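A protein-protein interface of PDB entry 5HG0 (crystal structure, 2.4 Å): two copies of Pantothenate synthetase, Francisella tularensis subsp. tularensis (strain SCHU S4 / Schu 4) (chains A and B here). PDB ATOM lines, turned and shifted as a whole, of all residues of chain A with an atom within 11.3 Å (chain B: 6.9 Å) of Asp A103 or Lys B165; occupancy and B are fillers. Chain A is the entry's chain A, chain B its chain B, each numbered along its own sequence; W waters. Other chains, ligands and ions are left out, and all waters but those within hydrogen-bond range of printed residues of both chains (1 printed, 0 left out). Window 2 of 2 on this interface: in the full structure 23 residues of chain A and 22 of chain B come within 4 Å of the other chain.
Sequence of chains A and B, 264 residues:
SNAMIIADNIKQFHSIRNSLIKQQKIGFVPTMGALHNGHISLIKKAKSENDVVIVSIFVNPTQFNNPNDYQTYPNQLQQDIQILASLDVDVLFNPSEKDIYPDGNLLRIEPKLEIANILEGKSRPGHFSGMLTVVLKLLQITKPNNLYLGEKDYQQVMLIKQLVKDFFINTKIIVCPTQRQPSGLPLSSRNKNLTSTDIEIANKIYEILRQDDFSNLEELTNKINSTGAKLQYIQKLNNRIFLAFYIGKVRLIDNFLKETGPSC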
ATOM      1  N   ILE A  10      11.105   0.323   4.037  1.00  0.00           N
ATOM      2  CA  ILE A  10      12.548   0.301   3.815  1.00  0.00           C
ATOM      3  C   ILE A  10      12.865   0.036   2.347  1.00  0.00           C
ATOM      4  O   ILE A  10      13.679   0.741   1.736  1.00  0.00           O
ATOM      5  CB  ILE A  10      13.212  -0.745   4.728  1.00  0.00           C
ATOM      6  CG1 ILE A  10      13.003  -0.384   6.199  1.00  0.00           C
ATOM      7  CG2 ILE A  10      14.691  -0.854   4.423  1.00  0.00           C
ATOM      8  CD1 ILE A  10      13.796   0.816   6.654  1.00  0.00           C
ATOM      9  N   HIS A  14      15.179   2.327  -0.153  1.00  0.00           N
ATOM     10  CA  HIS A  14      16.427   1.887  -0.770  1.00  0.00           C
ATOM     11  C   HIS A  14      16.395   2.070  -2.280  1.00  0.00           C
ATOM     12  O   HIS A  14      17.442   2.288  -2.901  1.00  0.00           O
ATOM     13  CB  HIS A  14      16.704   0.426  -0.416  1.00  0.00           C
ATOM     14  CG  HIS A  14      17.148   0.221   1.000  1.00  0.00           C
ATOM     15  ND1 HIS A  14      17.819   1.186   1.718  1.00  0.00           N
ATOM     16  CD2 HIS A  14      17.017  -0.842   1.829  1.00  0.00           C
ATOM     17  CE1 HIS A  14      18.083   0.726   2.929  1.00  0.00           C
ATOM     18  NE2 HIS A  14      17.607  -0.502   3.022  1.00  0.00           N
ATOM     19  N   PHE A  58       8.860   9.591  12.145  1.00  0.00           N
ATOM     20  CA  PHE A  58       8.766   8.296  12.812  1.00  0.00           C
ATOM     21  C   PHE A  58       8.678   8.539  14.311  1.00  0.00           C
ATOM     22  O   PHE A  58       9.664   8.957  14.929  1.00  0.00           O
ATOM     23  CB  PHE A  58       9.966   7.422  12.461  1.00  0.00           C
ATOM     24  CG  PHE A  58      10.004   6.119  13.201  1.00  0.00           C
ATOM     25  CD1 PHE A  58       9.048   5.144  12.962  1.00  0.00           C
ATOM     26  CD2 PHE A  58      10.998   5.863  14.128  1.00  0.00           C
ATOM     27  CE1 PHE A  58       9.081   3.939  13.641  1.00  0.00           C
ATOM     28  CE2 PHE A  58      11.038   4.660  14.811  1.00  0.00           C
ATOM     29  CZ  PHE A  58      10.075   3.697  14.566  1.00  0.00           C
ATOM     30  N   THR A  62      10.694   3.504  21.359  1.00  0.00           N
ATOM     31  CA  THR A  62      11.684   3.054  22.329  1.00  0.00           C
ATOM     32  C   THR A  62      12.340   4.194  23.100  1.00  0.00           C
ATOM     33  O   THR A  62      13.079   3.922  24.053  1.00  0.00           O
ATOM     34  CB  THR A  62      12.765   2.229  21.628  1.00  0.00           C
ATOM     35  OG1 THR A  62      13.580   1.572  22.604  1.00  0.00           O
ATOM     36  CG2 THR A  62      13.643   3.129  20.788  1.00  0.00           C
ATOM     37  N   SER A  96       7.253   2.362   9.341  1.00  0.00           N
ATOM     38  CA  SER A  96       6.481   1.767  10.416  1.00  0.00           C
ATOM     39  C   SER A  96       7.412   1.229  11.500  1.00  0.00           C
ATOM     40  O   SER A  96       8.636   1.208  11.355  1.00  0.00           O
ATOM     41  CB  SER A  96       5.589   0.648   9.881  1.00  0.00           C
ATOM     42  OG  SER A  96       6.354  -0.502   9.575  1.00  0.00           O
ATOM     43  N   GLU A  97       6.806   0.778  12.601  1.00  0.00           N
ATOM     44  CA  GLU A  97       7.591   0.241  13.707  1.00  0.00           C
ATOM     45  C   GLU A  97       8.302  -1.044  13.300  1.00  0.00           C
ATOM     46  O   GLU A  97       9.471  -1.254  13.647  1.00  0.00           O
ATOM     47  CB  GLU A  97       6.683   0.004  14.913  1.00  0.00           C
ATOM     48  CG  GLU A  97       7.405  -0.116  16.242  1.00  0.00           C
ATOM     49  CD  GLU A  97       6.441  -0.188  17.414  1.00  0.00           C
ATOM     50  OE1 GLU A  97       5.335   0.385  17.312  1.00  0.00           O
ATOM     51  OE2 GLU A  97       6.786  -0.820  18.436  1.00  0.00           O
ATOM     52  N   LYS A  98       7.614  -1.912  12.553  1.00  0.00           N
ATOM     53  CA  LYS A  98       8.234  -3.143  12.076  1.00  0.00           C
ATOM     54  C   LYS A  98       9.400  -2.862  11.137  1.00  0.00           C
ATOM     55  O   LYS A  98      10.369  -3.628  11.105  1.00  0.00           O
ATOM     56  CB  LYS A  98       7.193  -4.016  11.373  1.00  0.00           C
ATOM     57  CG  LYS A  98       6.159  -4.638  12.298  1.00  0.00           C
ATOM     58  CD  LYS A  98       4.971  -5.213  11.521  1.00  0.00           C
ATOM     59  CE  LYS A  98       5.381  -6.363  10.604  1.00  0.00           C
ATOM     60  NZ  LYS A  98       5.796  -5.912   9.244  1.00  0.00           N
ATOM     61  N   ASP A  99       9.325  -1.775  10.364  1.00  0.00           N
ATOM     62  CA  ASP A  99      10.421  -1.437   9.462  1.00  0.00           C
ATOM     63  C   ASP A  99      11.700  -1.137  10.233  1.00  0.00           C
ATOM     64  O   ASP A  99      12.785  -1.603   9.861  1.00  0.00           O
ATOM     65  CB  ASP A  99      10.037  -0.243   8.588  1.00  0.00           C
ATOM     66  CG  ASP A  99       9.038  -0.604   7.512  1.00  0.00           C
ATOM     67  OD1 ASP A  99       8.940  -1.805   7.176  1.00  0.00           O
ATOM     68  OD2 ASP A  99       8.366   0.317   7.001  1.00  0.00           O
ATOM     69  N   ILE A 100      11.593  -0.361  11.310  1.00  0.00           N
ATOM     70  CA  ILE A 100      12.769   0.016  12.083  1.00  0.00           C
ATOM     71  C   ILE A 100      13.175  -1.060  13.087  1.00  0.00           C
ATOM     72  O   ILE A 100      14.371  -1.251  13.338  1.00  0.00           O
ATOM     73  CB  ILE A 100      12.514   1.362  12.784  1.00  0.00           C
ATOM     74  CG1 ILE A 100      12.152   2.434  11.751  1.00  0.00           C
ATOM     75  CG2 ILE A 100      13.734   1.799  13.570  1.00  0.00           C
ATOM     76  CD1 ILE A 100      13.208   2.605  10.675  1.00  0.00           C
ATOM     77  N   TYR A 101      12.211  -1.777  13.668  1.00  0.00           N
ATOM     78  CA  TYR A 101      12.483  -2.846  14.626  1.00  0.00           C
ATOM     79  C   TYR A 101      11.813  -4.119  14.128  1.00  0.00           C
ATOM     80  O   TYR A 101      10.729  -4.489  14.597  1.00  0.00           O
ATOM     81  CB  TYR A 101      12.005  -2.470  16.031  1.00  0.00           C
ATOM     82  CG  TYR A 101      12.594  -1.169  16.527  1.00  0.00           C
ATOM     83  CD1 TYR A 101      13.846  -1.137  17.126  1.00  0.00           C
ATOM     84  CD2 TYR A 101      11.909   0.028  16.373  1.00  0.00           C
ATOM     85  CE1 TYR A 101      14.397   0.049  17.565  1.00  0.00           C
ATOM     86  CE2 TYR A 101      12.449   1.218  16.812  1.00  0.00           C
ATOM     87  CZ  TYR A 101      13.694   1.224  17.406  1.00  0.00           C
ATOM     88  OH  TYR A 101      14.241   2.408  17.842  1.00  0.00           O
ATOM     89  N   PRO A 102      12.434  -4.817  13.172  1.00  0.00           N
ATOM     90  CA  PRO A 102      11.807  -6.043  12.646  1.00  0.00           C
ATOM     91  C   PRO A 102      11.661  -7.142  13.685  1.00  0.00           C
ATOM     92  O   PRO A 102      10.673  -7.888  13.658  1.00  0.00           O
ATOM     93  CB  PRO A 102      12.752  -6.453  11.507  1.00  0.00           C
ATOM     94  CG  PRO A 102      14.059  -5.824  11.851  1.00  0.00           C
ATOM     95  CD  PRO A 102      13.722  -4.526  12.518  1.00  0.00           C
ATOM     96  N   ASP A 103      12.616  -7.259  14.606  1.00  0.00           N
ATOM     97  CA  ASP A 103      12.592  -8.286  15.639  1.00  0.00           C
ATOM     98  C   ASP A 103      12.423  -7.700  17.036  1.00  0.00           C
ATOM     99  O   ASP A 103      12.743  -8.366  18.024  1.00  0.00           O
ATOM    100  CB  ASP A 103      13.867  -9.128  15.575  1.00  0.00           C
ATOM    101  CG  ASP A 103      14.056  -9.799  14.230  1.00  0.00           C
ATOM    102  OD1 ASP A 103      13.059 -10.299  13.669  1.00  0.00           O
ATOM    103  OD2 ASP A 103      15.199  -9.815  13.728  1.00  0.00           O
ATOM    104  N   GLY A 104      11.922  -6.476  17.140  1.00  0.00           N
ATOM    105  CA  GLY A 104      11.812  -5.819  18.424  1.00  0.00           C
ATOM    106  C   GLY A 104      13.018  -4.958  18.736  1.00  0.00           C
ATOM    107  O   GLY A 104      13.873  -4.678  17.890  1.00  0.00           O
ATOM    108  N   ASN A 105      13.081  -4.528  19.994  1.00  0.00           N
ATOM    109  CA  ASN A 105      14.157  -3.655  20.458  1.00  0.00           C
ATOM    110  C   ASN A 105      15.197  -4.486  21.211  1.00  0.00           C
ATOM    111  O   ASN A 105      15.363  -4.396  22.430  1.00  0.00           O
ATOM    112  CB  ASN A 105      13.589  -2.532  21.320  1.00  0.00           C
ATOM    113  CG  ASN A 105      14.637  -1.512  21.713  1.00  0.00           C
ATOM    114  OD1 ASN A 105      14.614  -0.978  22.821  1.00  0.00           O
ATOM    115  ND2 ASN A 105      15.572  -1.243  20.809  1.00  0.00           N
ATOM    116  N   LEU A 106      15.920  -5.300  20.441  1.00  0.00           N
ATOM    117  CA  LEU A 106      16.830  -6.292  21.000  1.00  0.00           C
ATOM    118  C   LEU A 106      18.241  -5.754  21.218  1.00  0.00           C
ATOM    119  O   LEU A 106      18.845  -6.019  22.261  1.00  0.00           O
ATOM    120  CB  LEU A 106      16.882  -7.521  20.089  1.00  0.00           C
ATOM    121  CG  LEU A 106      15.538  -8.183  19.777  1.00  0.00           C
ATOM    122  CD1 LEU A 106      15.732  -9.373  18.852  1.00  0.00           C
ATOM    123  CD2 LEU A 106      14.825  -8.602  21.057  1.00  0.00           C
ATOM    124  N   LEU A 107      18.785  -5.012  20.254  1.00  0.00           N
ATOM    125  CA  LEU A 107      20.140  -4.470  20.337  1.00  0.00           C
ATOM    126  C   LEU A 107      20.046  -2.957  20.494  1.00  0.00           C
ATOM    127  O   LEU A 107      19.574  -2.261  19.589  1.00  0.00           O
ATOM    128  CB  LEU A 107      20.958  -4.843  19.103  1.00  0.00           C
ATOM    129  CG  LEU A 107      21.178  -6.340  18.882  1.00  0.00           C
ATOM    130  CD1 LEU A 107      21.930  -6.577  17.596  1.00  0.00           C
ATOM    131  CD2 LEU A 107      21.920  -6.957  20.055  1.00  0.00           C
ATOM    132  N   ARG A 108      20.510  -2.450  21.633  1.00  0.00           N
ATOM    133  CA  ARG A 108      20.327  -1.054  22.001  1.00  0.00           C
ATOM    134  C   ARG A 108      21.673  -0.380  22.219  1.00  0.00           C
ATOM    135  O   ARG A 108      22.605  -0.990  22.754  1.00  0.00           O
ATOM    136  CB  ARG A 108      19.481  -0.938  23.272  1.00  0.00           C
ATOM    137  CG  ARG A 108      18.296  -1.879  23.285  1.00  0.00           C
ATOM    138  CD  ARG A 108      17.630  -1.925  24.645  1.00  0.00           C
ATOM    139  NE  ARG A 108      16.544  -2.901  24.662  1.00  0.00           N
ATOM    140  CZ  ARG A 108      15.645  -3.009  25.634  1.00  0.00           C
ATOM    141  NH1 ARG A 108      15.693  -2.193  26.680  1.00  0.00           N
ATOM    142  NH2 ARG A 108      14.694  -3.930  25.556  1.00  0.00           N
ATOM    143  N   THR A 133      19.653   4.801  19.491  1.00  0.00           N
ATOM    144  CA  THR A 133      19.456   3.581  18.715  1.00  0.00           C
ATOM    145  C   THR A 133      18.744   3.881  17.401  1.00  0.00           C
ATOM    146  O   THR A 133      19.179   3.436  16.332  1.00  0.00           O
ATOM    147  CB  THR A 133      18.670   2.553  19.531  1.00  0.00           C
ATOM    148  OG1 THR A 133      19.404   2.207  20.713  1.00  0.00           O
ATOM    149  CG2 THR A 133      18.427   1.292  18.709  1.00  0.00           C
ATOM    150  N   LEU A 136      20.993   6.027  15.036  1.00  0.00           N
ATOM    151  CA  LEU A 136      21.960   5.179  14.349  1.00  0.00           C
ATOM    152  C   LEU A 136      21.295   4.405  13.217  1.00  0.00           C
ATOM    153  O   LEU A 136      21.823   4.341  12.101  1.00  0.00           O
ATOM    154  CB  LEU A 136      22.626   4.230  15.345  1.00  0.00           C
ATOM    155  CG  LEU A 136      23.707   3.301  14.788  1.00  0.00           C
ATOM    156  CD1 LEU A 136      24.754   4.094  14.035  1.00  0.00           C
ATOM    157  CD2 LEU A 136      24.358   2.505  15.911  1.00  0.00           C
ATOM    158  N   LYS A 137      20.123   3.824  13.484  1.00  0.00           N
ATOM    159  CA  LYS A 137      19.381   3.124  12.437  1.00  0.00           C
ATOM    160  C   LYS A 137      19.036   4.059  11.284  1.00  0.00           C
ATOM    161  O   LYS A 137      19.231   3.716  10.111  1.00  0.00           O
ATOM    162  CB  LYS A 137      18.111   2.504  13.023  1.00  0.00           C
ATOM    163  CG  LYS A 137      18.342   1.265  13.873  1.00  0.00           C
ATOM    164  CD  LYS A 137      17.096   0.905  14.667  1.00  0.00           C
ATOM    165  CE  LYS A 137      17.236  -0.445  15.351  1.00  0.00           C
ATOM    166  NZ  LYS A 137      17.135  -1.579  14.394  1.00  0.00           N
ATOM    167  N   LEU A 138      18.520   5.249  11.601  1.00  0.00           N
ATOM    168  CA  LEU A 138      18.139   6.193  10.556  1.00  0.00           C
ATOM    169  C   LEU A 138      19.347   6.643   9.743  1.00  0.00           C
ATOM    170  O   LEU A 138      19.246   6.845   8.528  1.00  0.00           O
ATOM    171  CB  LEU A 138      17.424   7.396  11.173  1.00  0.00           C
ATOM    172  CG  LEU A 138      16.039   7.104  11.749  1.00  0.00           C
ATOM    173  CD1 LEU A 138      15.520   8.280  12.559  1.00  0.00           C
ATOM    174  CD2 LEU A 138      15.072   6.743  10.635  1.00  0.00           C
ATOM    175  N   GLN A 140      22.034   4.807   9.200  1.00  0.00           N
ATOM    176  CA  GLN A 140      22.429   3.678   8.363  1.00  0.00           C
ATOM    177  C   GLN A 140      21.523   3.537   7.146  1.00  0.00           C
ATOM    178  O   GLN A 140      21.980   3.103   6.084  1.00  0.00           O
ATOM    179  CB  GLN A 140      22.416   2.384   9.178  1.00  0.00           C
ATOM    180  CG  GLN A 140      23.396   2.357  10.342  1.00  0.00           C
ATOM    181  CD  GLN A 140      24.841   2.310   9.896  1.00  0.00           C
ATOM    182  OE1 GLN A 140      25.510   3.340   9.800  1.00  0.00           O
ATOM    183  NE2 GLN A 140      25.334   1.109   9.622  1.00  0.00           N
ATOM    184  N   ILE A 141      20.246   3.898   7.280  1.00  0.00           N
ATOM    185  CA  ILE A 141      19.307   3.776   6.169  1.00  0.00           C
ATOM    186  C   ILE A 141      19.518   4.894   5.155  1.00  0.00           C
ATOM    187  O   ILE A 141      19.646   4.645   3.951  1.00  0.00           O
ATOM    188  CB  ILE A 141      17.861   3.765   6.697  1.00  0.00           C
ATOM    189  CG1 ILE A 141      17.610   2.512   7.534  1.00  0.00           C
ATOM    190  CG2 ILE A 141      16.869   3.860   5.545  1.00  0.00           C
ATOM    191  CD1 ILE A 141      16.411   2.630   8.461  1.00  0.00           C
ATOM    192  N   LEU B 159      24.445 -13.302  17.280  1.00  0.00           N
ATOM    193  CA  LEU B 159      24.307 -11.907  17.685  1.00  0.00           C
ATOM    194  C   LEU B 159      24.788 -10.963  16.591  1.00  0.00           C
ATOM    195  O   LEU B 159      24.175  -9.914  16.354  1.00  0.00           O
ATOM    196  CB  LEU B 159      25.070 -11.658  18.986  1.00  0.00           C
ATOM    197  CG  LEU B 159      24.515 -12.344  20.235  1.00  0.00           C
ATOM    198  CD1 LEU B 159      25.457 -12.153  21.410  1.00  0.00           C
ATOM    199  CD2 LEU B 159      23.132 -11.810  20.573  1.00  0.00           C
ATOM    200  N   ILE B 160      25.878 -11.318  15.909  1.00  0.00           N
ATOM    201  CA  ILE B 160      26.381 -10.477  14.829  1.00  0.00           C
ATOM    202  C   ILE B 160      25.420 -10.497  13.646  1.00  0.00           C
ATOM    203  O   ILE B 160      25.223  -9.478  12.972  1.00  0.00           O
ATOM    204  CB  ILE B 160      27.799 -10.919  14.430  1.00  0.00           C
ATOM    205  CG1 ILE B 160      28.781 -10.615  15.563  1.00  0.00           C
ATOM    206  CG2 ILE B 160      28.245 -10.225  13.152  1.00  0.00           C
ATOM    207  CD1 ILE B 160      30.161 -11.188  15.341  1.00  0.00           C
ATOM    208  N   LYS B 161      24.806 -11.653  13.374  1.00  0.00           N
ATOM    209  CA  LYS B 161      23.745 -11.707  12.372  1.00  0.00           C
ATOM    210  C   LYS B 161      22.614 -10.751  12.727  1.00  0.00           C
ATOM    211  O   LYS B 161      22.094 -10.041  11.857  1.00  0.00           O
ATOM    212  CB  LYS B 161      23.213 -13.134  12.234  1.00  0.00           C
ATOM    213  CG  LYS B 161      24.077 -14.054  11.387  1.00  0.00           C
ATOM    214  CD  LYS B 161      23.486 -15.449  11.337  1.00  0.00           C
ATOM    215  CE  LYS B 161      24.298 -16.365  10.440  1.00  0.00           C
ATOM    216  NZ  LYS B 161      23.833 -17.780  10.526  1.00  0.00           N
ATOM    217  N   GLN B 162      22.222 -10.719  14.002  1.00  0.00           N
ATOM    218  CA  GLN B 162      21.227  -9.749  14.447  1.00  0.00           C
ATOM    219  C   GLN B 162      21.752  -8.326  14.305  1.00  0.00           C
ATOM    220  O   GLN B 162      21.008  -7.417  13.918  1.00  0.00           O
ATOM    221  CB  GLN B 162      20.832 -10.033  15.896  1.00  0.00           C
ATOM    222  CG  GLN B 162      19.652  -9.217  16.389  1.00  0.00           C
ATOM    223  CD  GLN B 162      18.366  -9.573  15.671  1.00  0.00           C
ATOM    224  OE1 GLN B 162      17.988 -10.743  15.592  1.00  0.00           O
ATOM    225  NE2 GLN B 162      17.691  -8.562  15.131  1.00  0.00           N
ATOM    226  N   LEU B 163      23.036  -8.118  14.610  1.00  0.00           N
ATOM    227  CA  LEU B 163      23.631  -6.788  14.511  1.00  0.00           C
ATOM    228  C   LEU B 163      23.571  -6.261  13.084  1.00  0.00           C
ATOM    229  O   LEU B 163      23.124  -5.135  12.841  1.00  0.00           O
ATOM    230  CB  LEU B 163      25.078  -6.830  15.005  1.00  0.00           C
ATOM    231  CG  LEU B 163      25.859  -5.513  15.023  1.00  0.00           C
ATOM    232  CD1 LEU B 163      25.472  -4.667  16.229  1.00  0.00           C
ATOM    233  CD2 LEU B 163      27.355  -5.776  14.996  1.00  0.00           C
ATOM    234  N   VAL B 164      24.027  -7.067  12.122  1.00  0.00           N
ATOM    235  CA  VAL B 164      24.033  -6.647  10.725  1.00  0.00           C
ATOM    236  C   VAL B 164      22.617  -6.345  10.249  1.00  0.00           C
ATOM    237  O   VAL B 164      22.394  -5.413   9.467  1.00  0.00           O
ATOM    238  CB  VAL B 164      24.715  -7.724   9.856  1.00  0.00           C
ATOM    239  CG1 VAL B 164      24.413  -7.513   8.381  1.00  0.00           C
ATOM    240  CG2 VAL B 164      26.222  -7.734  10.096  1.00  0.00           C
ATOM    241  N   LYS B 165      21.635  -7.112  10.729  1.00  0.00           N
ATOM    242  CA  LYS B 165      20.255  -6.901  10.303  1.00  0.00           C
ATOM    243  C   LYS B 165      19.668  -5.637  10.922  1.00  0.00           C
ATOM    244  O   LYS B 165      19.058  -4.817  10.225  1.00  0.00           O
ATOM    245  CB  LYS B 165      19.404  -8.121  10.661  1.00  0.00           C
ATOM    246  CG  LYS B 165      17.947  -8.002  10.242  1.00  0.00           C
ATOM    247  CD  LYS B 165      17.139  -9.211  10.680  1.00  0.00           C
ATOM    248  CE  LYS B 165      15.667  -9.044  10.331  1.00  0.00           C
ATOM    249  NZ  LYS B 165      14.841 -10.206  10.768  1.00  0.00           N
ATOM    250  N   ASP B 166      19.846  -5.458  12.233  1.00  0.00           N
ATOM    251  CA  ASP B 166      19.171  -4.369  12.933  1.00  0.00           C
ATOM    252  C   ASP B 166      19.728  -3.003  12.557  1.00  0.00           C
ATOM    253  O   ASP B 166      18.986  -2.015  12.559  1.00  0.00           O
ATOM    254  CB  ASP B 166      19.267  -4.577  14.443  1.00  0.00           C
ATOM    255  CG  ASP B 166      18.026  -5.222  15.019  1.00  0.00           C
ATOM    256  OD1 ASP B 166      16.910  -4.811  14.632  1.00  0.00           O
ATOM    257  OD2 ASP B 166      18.164  -6.144  15.850  1.00  0.00           O
ATOM    258  N   PHE B 167      21.021  -2.916  12.247  1.00  0.00           N
ATOM    259  CA  PHE B 167      21.633  -1.642  11.893  1.00  0.00           C
ATOM    260  C   PHE B 167      21.939  -1.544  10.404  1.00  0.00           C
ATOM    261  O   PHE B 167      22.778  -0.736   9.995  1.00  0.00           O
ATOM    262  CB  PHE B 167      22.881  -1.411  12.742  1.00  0.00           C
ATOM    263  CG  PHE B 167      22.579  -1.261  14.203  1.00  0.00           C
ATOM    264  CD1 PHE B 167      21.982  -0.103  14.682  1.00  0.00           C
ATOM    265  CD2 PHE B 167      22.865  -2.281  15.096  1.00  0.00           C
ATOM    266  CE1 PHE B 167      21.687   0.040  16.025  1.00  0.00           C
ATOM    267  CE2 PHE B 167      22.575  -2.146  16.441  1.00  0.00           C
ATOM    268  CZ  PHE B 167      21.985  -0.984  16.907  1.00  0.00           C
ATOM    269  N   PHE B 168      21.271  -2.367   9.593  1.00  0.00           N
ATOM    270  CA  PHE B 168      21.164  -2.170   8.149  1.00  0.00           C
ATOM    271  C   PHE B 168      22.534  -2.094   7.479  1.00  0.00           C
ATOM    272  O   PHE B 168      22.808  -1.217   6.657  1.00  0.00           O
ATOM    273  CB  PHE B 168      20.325  -0.928   7.848  1.00  0.00           C
ATOM    274  CG  PHE B 168      18.983  -0.940   8.521  1.00  0.00           C
ATOM    275  CD1 PHE B 168      17.915  -1.613   7.950  1.00  0.00           C
ATOM    276  CD2 PHE B 168      18.794  -0.289   9.731  1.00  0.00           C
ATOM    277  CE1 PHE B 168      16.678  -1.629   8.570  1.00  0.00           C
ATOM    278  CE2 PHE B 168      17.562  -0.302  10.358  1.00  0.00           C
ATOM    279  CZ  PHE B 168      16.502  -0.972   9.779  1.00  0.00           C
ATOM    280  N   ILE B 169      23.401  -3.032   7.843  1.00  0.00           N
ATOM    281  CA  ILE B 169      24.721  -3.160   7.240  1.00  0.00           C
ATOM    282  C   ILE B 169      24.610  -4.088   6.038  1.00  0.00           C
ATOM    283  O   ILE B 169      24.114  -5.214   6.154  1.00  0.00           O
ATOM    284  CB  ILE B 169      25.741  -3.689   8.262  1.00  0.00           C
ATOM    285  CG1 ILE B 169      25.986  -2.643   9.351  1.00  0.00           C
ATOM    286  CG2 ILE B 169      27.043  -4.073   7.575  1.00  0.00           C
ATOM    287  CD1 ILE B 169      26.665  -3.188  10.588  1.00  0.00           C
ATOM    288  N   ILE B 173      27.017 -12.610   5.691  1.00  0.00           N
ATOM    289  CA  ILE B 173      27.754 -13.297   6.745  1.00  0.00           C
ATOM    290  C   ILE B 173      27.933 -14.749   6.334  1.00  0.00           C
ATOM    291  O   ILE B 173      26.950 -15.470   6.123  1.00  0.00           O
ATOM    292  CB  ILE B 173      27.039 -13.188   8.099  1.00  0.00           C
ATOM    293  CG1 ILE B 173      27.014 -11.732   8.572  1.00  0.00           C
ATOM    294  CG2 ILE B 173      27.718 -14.083   9.121  1.00  0.00           C
ATOM    295  CD1 ILE B 173      26.305 -11.523   9.883  1.00  0.00           C
HETATM  296  O   HOH W   1      16.202 -12.882  13.862  1.00  0.00           O
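Water W1 bridges OD2 of Asp A103 (3.2 Å) and OE1 of Gln B162 (3.3 Å).
No position is printed for both chains. Of the 15 pairs that touch across the chains among the printed residues, none has its exchanged pair printed and touching as well.
Of the 23 printed residues of chain A, 8 touch a printed residue of chain B. Of the 12 printed residues of chain B, 7 touch a printed residue of chain A. Hydrophobic or aromatic side chains of chain B within 4 Å of the printed part of chain A: Phe B167, Phe B168 and Ile B169. Among the printed residues, 15 pairs touch across the chains. Among the printed residues, Asp or Glu carboxylates within 4 Å of a Lys or Arg side-chain nitrogen of the other chain: Asp A103 with Lys B165 and Lys A137 with Asp B166.
O of Ile A100 sits at hydrogen-bond distance from NZ of Lys A137, at 3.0 Å. The side-chain carboxylate (OD2) of Asp B166 is in hydrogen-bond range of the side-chain amide nitrogen (NE2) of Gln B162 (2.6 Å). The side-chain carboxylate of Asp A99 lies within hydrogen-bond range of the backbone NH of Ser A96 (3.3 Å). O of Val B164 lies within hydrogen-bond range of N of Ile B169 (3.1 Å).
Phe B168 touches Asp A99 (CZ to O, 3.8 Å). CG of Pro A102 touches CE of Lys B165, at 3.9 Å. OD1 of Asp B166 touches CD of Pro A102, at 3.8 Å. Leu A107 touches Gln B162 (CD1 to CG, 3.7 Å). Leu B163 touches Leu A107 (CA to CD1, 3.5 Å). O of Leu A107 touches CZ of Phe B167, 3.8 Å away. CD2 of Leu A136 touches CE1 of Phe B167, at 3.6 Å. Phe B167 touches Lys A137 (CD1 to CG, 3.97 Å). Phe B168 touches Lys A137 (CE2 to CB, 3.9 Å). Ile A141 touches Phe B168.
The side-chain carboxylate (OD2) of Asp A103 is in salt-bridge range of the side-chain amino group (NZ) of Lys B165. The side-chain amide nitrogen of Gln A140 sits close to the backbone carbonyl oxygen of Phe B167, 3.2 Å away. NZ of Lys A137 lies within salt-bridge range of OD1 of Asp B166, at 3.2 Å. OD2 of Asp A103 sits at hydrogen-bond distance from NE2 of Gln B162 (3.1 Å).
Asp A103 touches just these residues of chain B: Gln B162 (3.1 Å) and Lys B165 (3.0 Å). Of the printed residues of chain B, Leu A136 touches Phe B167. Printed residues of chain B within 4 Å of Gln A140: Phe B167 and Ile B169. Of the printed residues of chain B, Ile A141 touches Phe B168. Of the printed residues of chain A, Leu B163 touches Leu A107. No residue of chain A comes within 4 Å of Val B164. Lys B165 touches just these residues of chain A: Pro A102 and Asp A103. Of chain A, only Pro A102 and Lys A137 come within 4 Å of Asp B166. Of chain A, only Asp A99, Lys A137 and Ile A141 come within 4 Å of Phe B168. Of chain A, only Gln A140 comes within 4 Å of Ile B169. The nearest residue of chain A that does not touch Lys B165 is Lys A137 (5.6 Å). The nearest printed residue of chain B that does not touch Asp A99 is Asp B166 (6.8 Å).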
